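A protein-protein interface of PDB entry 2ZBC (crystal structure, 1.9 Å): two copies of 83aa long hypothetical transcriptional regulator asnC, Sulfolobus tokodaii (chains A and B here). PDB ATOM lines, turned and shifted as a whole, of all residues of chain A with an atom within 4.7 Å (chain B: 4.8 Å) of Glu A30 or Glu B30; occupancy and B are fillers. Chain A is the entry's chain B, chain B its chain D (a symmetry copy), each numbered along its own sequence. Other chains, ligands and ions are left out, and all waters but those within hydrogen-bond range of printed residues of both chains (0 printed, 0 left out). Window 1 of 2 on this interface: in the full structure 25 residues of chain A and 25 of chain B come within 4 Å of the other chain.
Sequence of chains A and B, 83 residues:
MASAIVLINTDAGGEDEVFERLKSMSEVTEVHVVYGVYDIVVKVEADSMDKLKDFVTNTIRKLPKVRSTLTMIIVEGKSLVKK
O of Val B31 lies within hydrogen-bond range of N of Leu A80 (2.8 Å).
The side-chain carboxylate (OE2) of Glu B30 sits close to the side-chain carboxylate (OE2) of Glu A30 (2.5 Å).
The backbone carbonyl oxygen (O) of Val A31 sits at hydrogen-bond distance from the backbone NH (N) of Leu B80, 2.9 Å away.
O of Thr A29 sits at hydrogen-bond distance from N of Lys B82.
OE1 of Glu A30 is in salt-bridge range of NZ of Lys B43, 3.2 Å away.
O of Val A28 is in hydrogen-bond range of NZ of Lys B82 (2.8 Å).
Thr A29 touches Val B81 (O to CA, 3.8 Å).
O of Leu B80 touches CA of Glu A30, at 3.1 Å.
Val B81 touches Glu A30.
His A32 touches Lys B43 (CE1 to NZ, 3.7 Å).
Leu B80 touches His A32 (O to CE1, 3.9 Å).
His A32 touches Val B81 (CE1 to CG2, 3.9 Å).
OE1 of Glu B30 touches CD of Lys A43 (3.3 Å).
Val A81 touches Thr B29.
CG2 of Val A81 touches OE1 of Glu B30 (3.7 Å).
Val A81 touches His B32 (CG2 to CE1, 3.9 Å).
Of the 11 printed residues of chain B, 8 touch a printed residue of chain A.
Printed residues of chain B that touch a printed residue of chain A: Thr B29, Glu B30, Val B31, His B32, Lys B43, Leu B80, Val B81 and Lys B82.
Hydrophobic or aromatic side chains of chain B that line the printed part of chain A: His B32 and Val B81.
Among the printed residues, 18 pairs touch across the chains.
Among the printed residues, Asp or Glu carboxylates within 4 Å of a Lys or Arg side-chain nitrogen of the other chain: Glu A30 with Lys B43.
O of Glu B30 sits at hydrogen-bond distance from N of Lys B43 (2.9 Å).
OE1 of Glu A30 sits at hydrogen-bond distance from NE2 of His A32.
N of Thr B29 lies within hydrogen-bond range of O of Lys B43 (2.9 Å).
The backbone carbonyl oxygen of Glu A30 lies within hydrogen-bond range of the backbone NH of Lys A43 (3.0 Å).
N of Val A41 sits at hydrogen-bond distance from O of His A32.
N of Thr A29 sits at hydrogen-bond distance from O of Lys A43, at 3.0 Å.
Glu A30 touches its own counterpart, Glu B30.
Glu A30 touches Lys B43, and with the chains exchanged Lys A43 touches Glu B30.
Glu A30 touches Val B81, and with the chains exchanged Val A81 touches Glu B30.
His A32 touches Lys B43, but with the chains exchanged Lys A43 does not touch His B32 (4.1 Å).
Positions printed for both chains: 28, 29, 30, 31, 32, 41, 42, 43, 80 and 81.
Of the 18 pairs that touch across the chains among the printed residues, 15 have their exchanged pair printed and touching as well.
Glu A30 touches four residues of chain B.
Printed residues of chain B within 4 Å of His A32: Lys B43 (3.7 Å), Leu B80 (3.9 Å) and Val B81 (3.9 Å).
Of the printed residues of chain B, Val A81 touches Thr B29 (3.8 Å), Glu B30 (3.7 Å) and His B32 (3.9 Å).
Glu B30 touches just these residues of chain A: Glu A30, Lys A43, Leu A80 and Val A81.
Of the printed residues of chain A, Leu B80 touches Glu A30, Val A31 and His A32.
Printed residues of chain A within 4 Å of Val B81: Thr A29 (3.8 Å), Glu A30 (3.9 Å) and His A32 (3.9 Å).
Of the printed residues of chain A, Lys B82 touches Val A28 (2.8 Å) and Thr A29 (2.9 Å).
The nearest printed residue of chain A that does not touch Glu B30 is Ile A5 (4.7 Å).
The nearest printed residue of chain A that does not touch Thr B29 is Leu A80 (4.4 Å).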
ATOM      1  N   ILE A   5       6.460 -11.430   0.743  1.00  0.00           N
ATOM      2  CA  ILE A   5       5.556 -10.940  -0.309  1.00  0.00           C
ATOM      3  C   ILE A   5       4.464 -10.200   0.455  1.00  0.00           C
ATOM      4  O   ILE A   5       3.871 -10.748   1.398  1.00  0.00           O
ATOM      5  CB  ILE A   5       4.976 -12.081  -1.116  1.00  0.00           C
ATOM      6  CG1 ILE A   5       6.066 -12.970  -1.797  1.00  0.00           C
ATOM      7  CG2 ILE A   5       3.986 -11.524  -2.178  1.00  0.00           C
ATOM      8  CD1 ILE A   5       6.968 -12.218  -2.620  1.00  0.00           C
ATOM      9  N   VAL A  28      12.016  -2.831  -2.265  1.00  0.00           N
ATOM     10  CA  VAL A  28      10.996  -3.362  -3.188  1.00  0.00           C
ATOM     11  C   VAL A  28      11.696  -3.878  -4.405  1.00  0.00           C
ATOM     12  O   VAL A  28      12.120  -3.095  -5.235  1.00  0.00           O
ATOM     13  CB  VAL A  28      10.000  -2.266  -3.537  1.00  0.00           C
ATOM     14  CG1 VAL A  28       9.063  -2.659  -4.744  1.00  0.00           C
ATOM     15  CG2 VAL A  28       9.175  -1.901  -2.328  1.00  0.00           C
ATOM     16  N   THR A  29      11.784  -5.201  -4.572  1.00  0.00           N
ATOM     17  CA  THR A  29      12.450  -5.784  -5.744  1.00  0.00           C
ATOM     18  C   THR A  29      11.520  -6.083  -6.900  1.00  0.00           C
ATOM     19  O   THR A  29      11.938  -6.296  -8.032  1.00  0.00           O
ATOM     20  CB  THR A  29      13.192  -7.056  -5.402  1.00  0.00           C
ATOM     21  OG1 THR A  29      12.284  -8.054  -4.881  1.00  0.00           O
ATOM     22  CG2 THR A  29      14.249  -6.801  -4.283  1.00  0.00           C
ATOM     23  N   GLU A  30      10.231  -6.127  -6.588  1.00  0.00           N
ATOM     24  CA  GLU A  30       9.238  -6.195  -7.630  1.00  0.00           C
ATOM     25  C   GLU A  30       7.894  -5.675  -7.065  1.00  0.00           C
ATOM     26  O   GLU A  30       7.666  -5.672  -5.857  1.00  0.00           O
ATOM     27  CB  GLU A  30       9.174  -7.631  -8.193  1.00  0.00           C
ATOM     28  CG  GLU A  30       8.360  -8.635  -7.459  1.00  0.00           C
ATOM     29  CD  GLU A  30       8.387 -10.011  -8.127  1.00  0.00           C
ATOM     30  OE1 GLU A  30       7.654 -10.211  -9.065  1.00  0.00           O
ATOM     31  OE2 GLU A  30       9.161 -10.874  -7.709  1.00  0.00           O
ATOM     32  N   VAL A  31       7.106  -5.085  -7.953  1.00  0.00           N
ATOM     33  CA  VAL A  31       5.844  -4.438  -7.584  1.00  0.00           C
ATOM     34  C   VAL A  31       4.863  -4.549  -8.816  1.00  0.00           C
ATOM     35  O   VAL A  31       5.257  -4.321  -9.988  1.00  0.00           O
ATOM     36  CB  VAL A  31       6.025  -3.033  -7.063  1.00  0.00           C
ATOM     37  CG1 VAL A  31       6.767  -2.148  -8.092  1.00  0.00           C
ATOM     38  CG2 VAL A  31       4.713  -2.425  -6.712  1.00  0.00           C
ATOM     39  N   HIS A  32       3.599  -4.897  -8.523  1.00  0.00           N
ATOM     40  CA  HIS A  32       2.640  -5.129  -9.574  1.00  0.00           C
ATOM     41  C   HIS A  32       1.298  -4.718  -9.085  1.00  0.00           C
ATOM     42  O   HIS A  32       0.894  -5.102  -7.985  1.00  0.00           O
ATOM     43  CB  HIS A  32       2.524  -6.619  -9.936  1.00  0.00           C
ATOM     44  CG  HIS A  32       3.832  -7.343 -10.044  1.00  0.00           C
ATOM     45  ND1 HIS A  32       4.522  -7.411 -11.224  1.00  0.00           N
ATOM     46  CD2 HIS A  32       4.562  -8.048  -9.137  1.00  0.00           C
ATOM     47  CE1 HIS A  32       5.643  -8.086 -11.033  1.00  0.00           C
ATOM     48  NE2 HIS A  32       5.669  -8.524  -9.786  1.00  0.00           N
ATOM     49  N   VAL A  41       0.920  -6.168  -5.323  1.00  0.00           N
ATOM     50  CA  VAL A  41       1.757  -7.189  -4.810  1.00  0.00           C
ATOM     51  C   VAL A  41       3.231  -6.687  -4.867  1.00  0.00           C
ATOM     52  O   VAL A  41       3.655  -6.219  -5.924  1.00  0.00           O
ATOM     53  CB  VAL A  41       1.623  -8.474  -5.636  1.00  0.00           C
ATOM     54  CG1 VAL A  41       2.543  -9.567  -5.084  1.00  0.00           C
ATOM     55  CG2 VAL A  41       0.192  -8.982  -5.646  1.00  0.00           C
ATOM     56  N   VAL A  42       3.937  -6.718  -3.747  1.00  0.00           N
ATOM     57  CA  VAL A  42       5.332  -6.312  -3.664  1.00  0.00           C
ATOM     58  C   VAL A  42       6.159  -7.452  -3.083  1.00  0.00           C
ATOM     59  O   VAL A  42       5.707  -8.141  -2.191  1.00  0.00           O
ATOM     60  CB  VAL A  42       5.572  -4.968  -2.815  1.00  0.00           C
ATOM     61  CG1 VAL A  42       5.188  -5.051  -1.462  1.00  0.00           C
ATOM     62  CG2 VAL A  42       6.970  -4.671  -2.699  1.00  0.00           C
ATOM     63  N   LYS A  43       7.334  -7.675  -3.604  1.00  0.00           N
ATOM     64  CA  LYS A  43       8.304  -8.507  -2.933  1.00  0.00           C
ATOM     65  C   LYS A  43       9.300  -7.573  -2.284  1.00  0.00           C
ATOM     66  O   LYS A  43       9.785  -6.661  -2.944  1.00  0.00           O
ATOM     67  CB  LYS A  43       9.038  -9.356  -3.938  1.00  0.00           C
ATOM     68  CG  LYS A  43       9.895 -10.394  -3.298  1.00  0.00           C
ATOM     69  CD  LYS A  43      10.279 -11.547  -4.271  1.00  0.00           C
ATOM     70  CE  LYS A  43      11.795 -11.712  -4.303  1.00  0.00           C
ATOM     71  NZ  LYS A  43      12.270 -12.796  -3.375  1.00  0.00           N
ATOM     72  N   LEU A  80      12.283 -19.815  -4.438  1.00  0.00           N
ATOM     73  CA  LEU A  80      13.138 -19.764  -5.640  1.00  0.00           C
ATOM     74  C   LEU A  80      12.695 -18.666  -6.550  1.00  0.00           C
ATOM     75  O   LEU A  80      11.497 -18.568  -6.857  1.00  0.00           O
ATOM     76  CB  LEU A  80      13.042 -21.093  -6.378  1.00  0.00           C
ATOM     77  CG  LEU A  80      13.577 -21.020  -7.817  1.00  0.00           C
ATOM     78  CD1 LEU A  80      15.112 -20.855  -7.768  1.00  0.00           C
ATOM     79  CD2 LEU A  80      13.161 -22.225  -8.534  1.00  0.00           C
ATOM     80  N   VAL A  81      13.629 -17.808  -6.950  1.00  0.00           N
ATOM     81  CA  VAL A  81      13.439 -16.872  -8.054  1.00  0.00           C
ATOM     82  C   VAL A  81      14.393 -17.276  -9.195  1.00  0.00           C
ATOM     83  O   VAL A  81      15.597 -17.228  -9.021  1.00  0.00           O
ATOM     84  CB  VAL A  81      13.724 -15.378  -7.614  1.00  0.00           C
ATOM     85  CG1 VAL A  81      13.643 -14.403  -8.778  1.00  0.00           C
ATOM     86  CG2 VAL A  81      12.764 -14.932  -6.505  1.00  0.00           C
ATOM     87  N   VAL B  28       6.579 -21.231 -14.251  1.00  0.00           N
ATOM     88  CA  VAL B  28       6.763 -20.740 -12.897  1.00  0.00           C
ATOM     89  C   VAL B  28       8.107 -19.969 -12.825  1.00  0.00           C
ATOM     90  O   VAL B  28       9.154 -20.564 -12.958  1.00  0.00           O
ATOM     91  CB  VAL B  28       6.672 -21.885 -11.836  1.00  0.00           C
ATOM     92  CG1 VAL B  28       7.058 -21.386 -10.448  1.00  0.00           C
ATOM     93  CG2 VAL B  28       5.279 -22.481 -11.807  1.00  0.00           C
ATOM     94  N   THR B  29       8.068 -18.647 -12.635  1.00  0.00           N
ATOM     95  CA  THR B  29       9.328 -17.863 -12.654  1.00  0.00           C
ATOM     96  C   THR B  29       9.835 -17.637 -11.260  1.00  0.00           C
ATOM     97  O   THR B  29      10.999 -17.282 -11.011  1.00  0.00           O
ATOM     98  CB  THR B  29       9.171 -16.595 -13.464  1.00  0.00           C
ATOM     99  OG1 THR B  29       8.187 -15.753 -12.848  1.00  0.00           O
ATOM    100  CG2 THR B  29       8.673 -16.886 -14.898  1.00  0.00           C
ATOM    101  N   GLU B  30       8.937 -17.779 -10.310  1.00  0.00           N
ATOM    102  CA  GLU B  30       9.297 -17.787  -8.928  1.00  0.00           C
ATOM    103  C   GLU B  30       8.184 -18.505  -8.107  1.00  0.00           C
ATOM    104  O   GLU B  30       7.005 -18.570  -8.543  1.00  0.00           O
ATOM    105  CB  GLU B  30       9.582 -16.314  -8.493  1.00  0.00           C
ATOM    106  CG  GLU B  30       8.453 -15.471  -7.952  1.00  0.00           C
ATOM    107  CD  GLU B  30       8.920 -14.084  -7.566  1.00  0.00           C
ATOM    108  OE1 GLU B  30       9.210 -13.887  -6.373  1.00  0.00           O
ATOM    109  OE2 GLU B  30       9.097 -13.221  -8.474  1.00  0.00           O
ATOM    110  N   VAL B  31       8.575 -19.097  -7.002  1.00  0.00           N
ATOM    111  CA  VAL B  31       7.684 -19.886  -6.098  1.00  0.00           C
ATOM    112  C   VAL B  31       8.234 -19.887  -4.688  1.00  0.00           C
ATOM    113  O   VAL B  31       9.474 -19.931  -4.481  1.00  0.00           O
ATOM    114  CB  VAL B  31       7.465 -21.283  -6.637  1.00  0.00           C
ATOM    115  CG1 VAL B  31       8.734 -22.097  -6.778  1.00  0.00           C
ATOM    116  CG2 VAL B  31       6.430 -22.059  -5.885  1.00  0.00           C
ATOM    117  N   HIS B  32       7.332 -19.752  -3.699  1.00  0.00           N
ATOM    118  CA  HIS B  32       7.695 -19.562  -2.297  1.00  0.00           C
ATOM    119  C   HIS B  32       6.620 -20.188  -1.427  1.00  0.00           C
ATOM    120  O   HIS B  32       5.454 -19.963  -1.698  1.00  0.00           O
ATOM    121  CB  HIS B  32       7.744 -18.085  -1.919  1.00  0.00           C
ATOM    122  CG  HIS B  32       8.473 -17.200  -2.874  1.00  0.00           C
ATOM    123  ND1 HIS B  32       9.844 -17.141  -2.906  1.00  0.00           N
ATOM    124  CD2 HIS B  32       8.038 -16.253  -3.748  1.00  0.00           C
ATOM    125  CE1 HIS B  32      10.222 -16.282  -3.828  1.00  0.00           C
ATOM    126  NE2 HIS B  32       9.152 -15.737  -4.365  1.00  0.00           N
ATOM    127  N   VAL B  41       3.017 -18.856  -2.857  1.00  0.00           N
ATOM    128  CA  VAL B  41       2.882 -17.816  -3.854  1.00  0.00           C
ATOM    129  C   VAL B  41       3.712 -18.198  -5.050  1.00  0.00           C
ATOM    130  O   VAL B  41       4.922 -18.518  -4.934  1.00  0.00           O
ATOM    131  CB  VAL B  41       3.351 -16.434  -3.301  1.00  0.00           C
ATOM    132  CG1 VAL B  41       3.139 -15.305  -4.335  1.00  0.00           C
ATOM    133  CG2 VAL B  41       2.679 -16.148  -1.999  1.00  0.00           C
ATOM    134  N   VAL B  42       3.100 -18.043  -6.233  1.00  0.00           N
ATOM    135  CA  VAL B  42       3.763 -18.344  -7.453  1.00  0.00           C
ATOM    136  C   VAL B  42       3.622 -17.187  -8.448  1.00  0.00           C
ATOM    137  O   VAL B  42       2.586 -16.533  -8.474  1.00  0.00           O
ATOM    138  CB  VAL B  42       3.155 -19.648  -8.138  1.00  0.00           C
ATOM    139  CG1 VAL B  42       4.000 -20.006  -9.278  1.00  0.00           C
ATOM    140  CG2 VAL B  42       3.121 -20.792  -7.187  1.00  0.00           C
ATOM    141  N   LYS B  43       4.663 -16.922  -9.231  1.00  0.00           N
ATOM    142  CA  LYS B  43       4.568 -16.011 -10.341  1.00  0.00           C
ATOM    143  C   LYS B  43       4.551 -16.846 -11.571  1.00  0.00           C
ATOM    144  O   LYS B  43       5.419 -17.707 -11.807  1.00  0.00           O
ATOM    145  CB  LYS B  43       5.690 -14.982 -10.376  1.00  0.00           C
ATOM    146  CG  LYS B  43       5.444 -13.937 -11.476  1.00  0.00           C
ATOM    147  CD  LYS B  43       6.344 -12.756 -11.255  1.00  0.00           C
ATOM    148  CE  LYS B  43       6.422 -11.855 -12.499  1.00  0.00           C
ATOM    149  NZ  LYS B  43       7.580 -10.955 -12.225  1.00  0.00           N
ATOM    150  N   LEU B  80       6.740  -4.187 -12.460  1.00  0.00           N
ATOM    151  CA  LEU B  80       8.203  -4.011 -12.402  1.00  0.00           C
ATOM    152  C   LEU B  80       8.872  -5.158 -11.663  1.00  0.00           C
ATOM    153  O   LEU B  80       8.494  -5.485 -10.537  1.00  0.00           O
ATOM    154  CB  LEU B  80       8.560  -2.687 -11.711  1.00  0.00           C
ATOM    155  CG  LEU B  80      10.091  -2.385 -11.562  1.00  0.00           C
ATOM    156  CD1 LEU B  80      10.792  -2.371 -12.873  1.00  0.00           C
ATOM    157  CD2 LEU B  80      10.238  -1.063 -10.850  1.00  0.00           C
ATOM    158  N   VAL B  81       9.889  -5.756 -12.295  1.00  0.00           N
ATOM    159  CA  VAL B  81      10.795  -6.672 -11.663  1.00  0.00           C
ATOM    160  C   VAL B  81      12.165  -6.052 -11.843  1.00  0.00           C
ATOM    161  O   VAL B  81      12.664  -5.941 -12.967  1.00  0.00           O
ATOM    162  CB  VAL B  81      10.748  -8.006 -12.349  1.00  0.00           C
ATOM    163  CG1 VAL B  81      11.724  -9.029 -11.749  1.00  0.00           C
ATOM    164  CG2 VAL B  81       9.296  -8.559 -12.352  1.00  0.00           C
ATOM    165  N   LYS B  82      12.784  -5.662 -10.749  1.00  0.00           N
ATOM    166  CA  LYS B  82      14.095  -5.013 -10.843  1.00  0.00           C
ATOM    167  C   LYS B  82      15.194  -5.987 -11.184  1.00  0.00           C
ATOM    168  O   LYS B  82      15.083  -7.194 -10.878  1.00  0.00           O
ATOM    169  CB  LYS B  82      14.380  -4.223  -9.583  1.00  0.00           C
ATOM    170  CG  LYS B  82      13.357  -3.154  -9.359  1.00  0.00           C
ATOM    171  CD  LYS B  82      13.594  -2.459  -8.062  1.00  0.00           C
ATOM    172  CE  LYS B  82      12.581  -1.431  -7.759  1.00  0.00           C
ATOM    173  NZ  LYS B  82      12.944  -0.730  -6.505  1.00  0.00           N
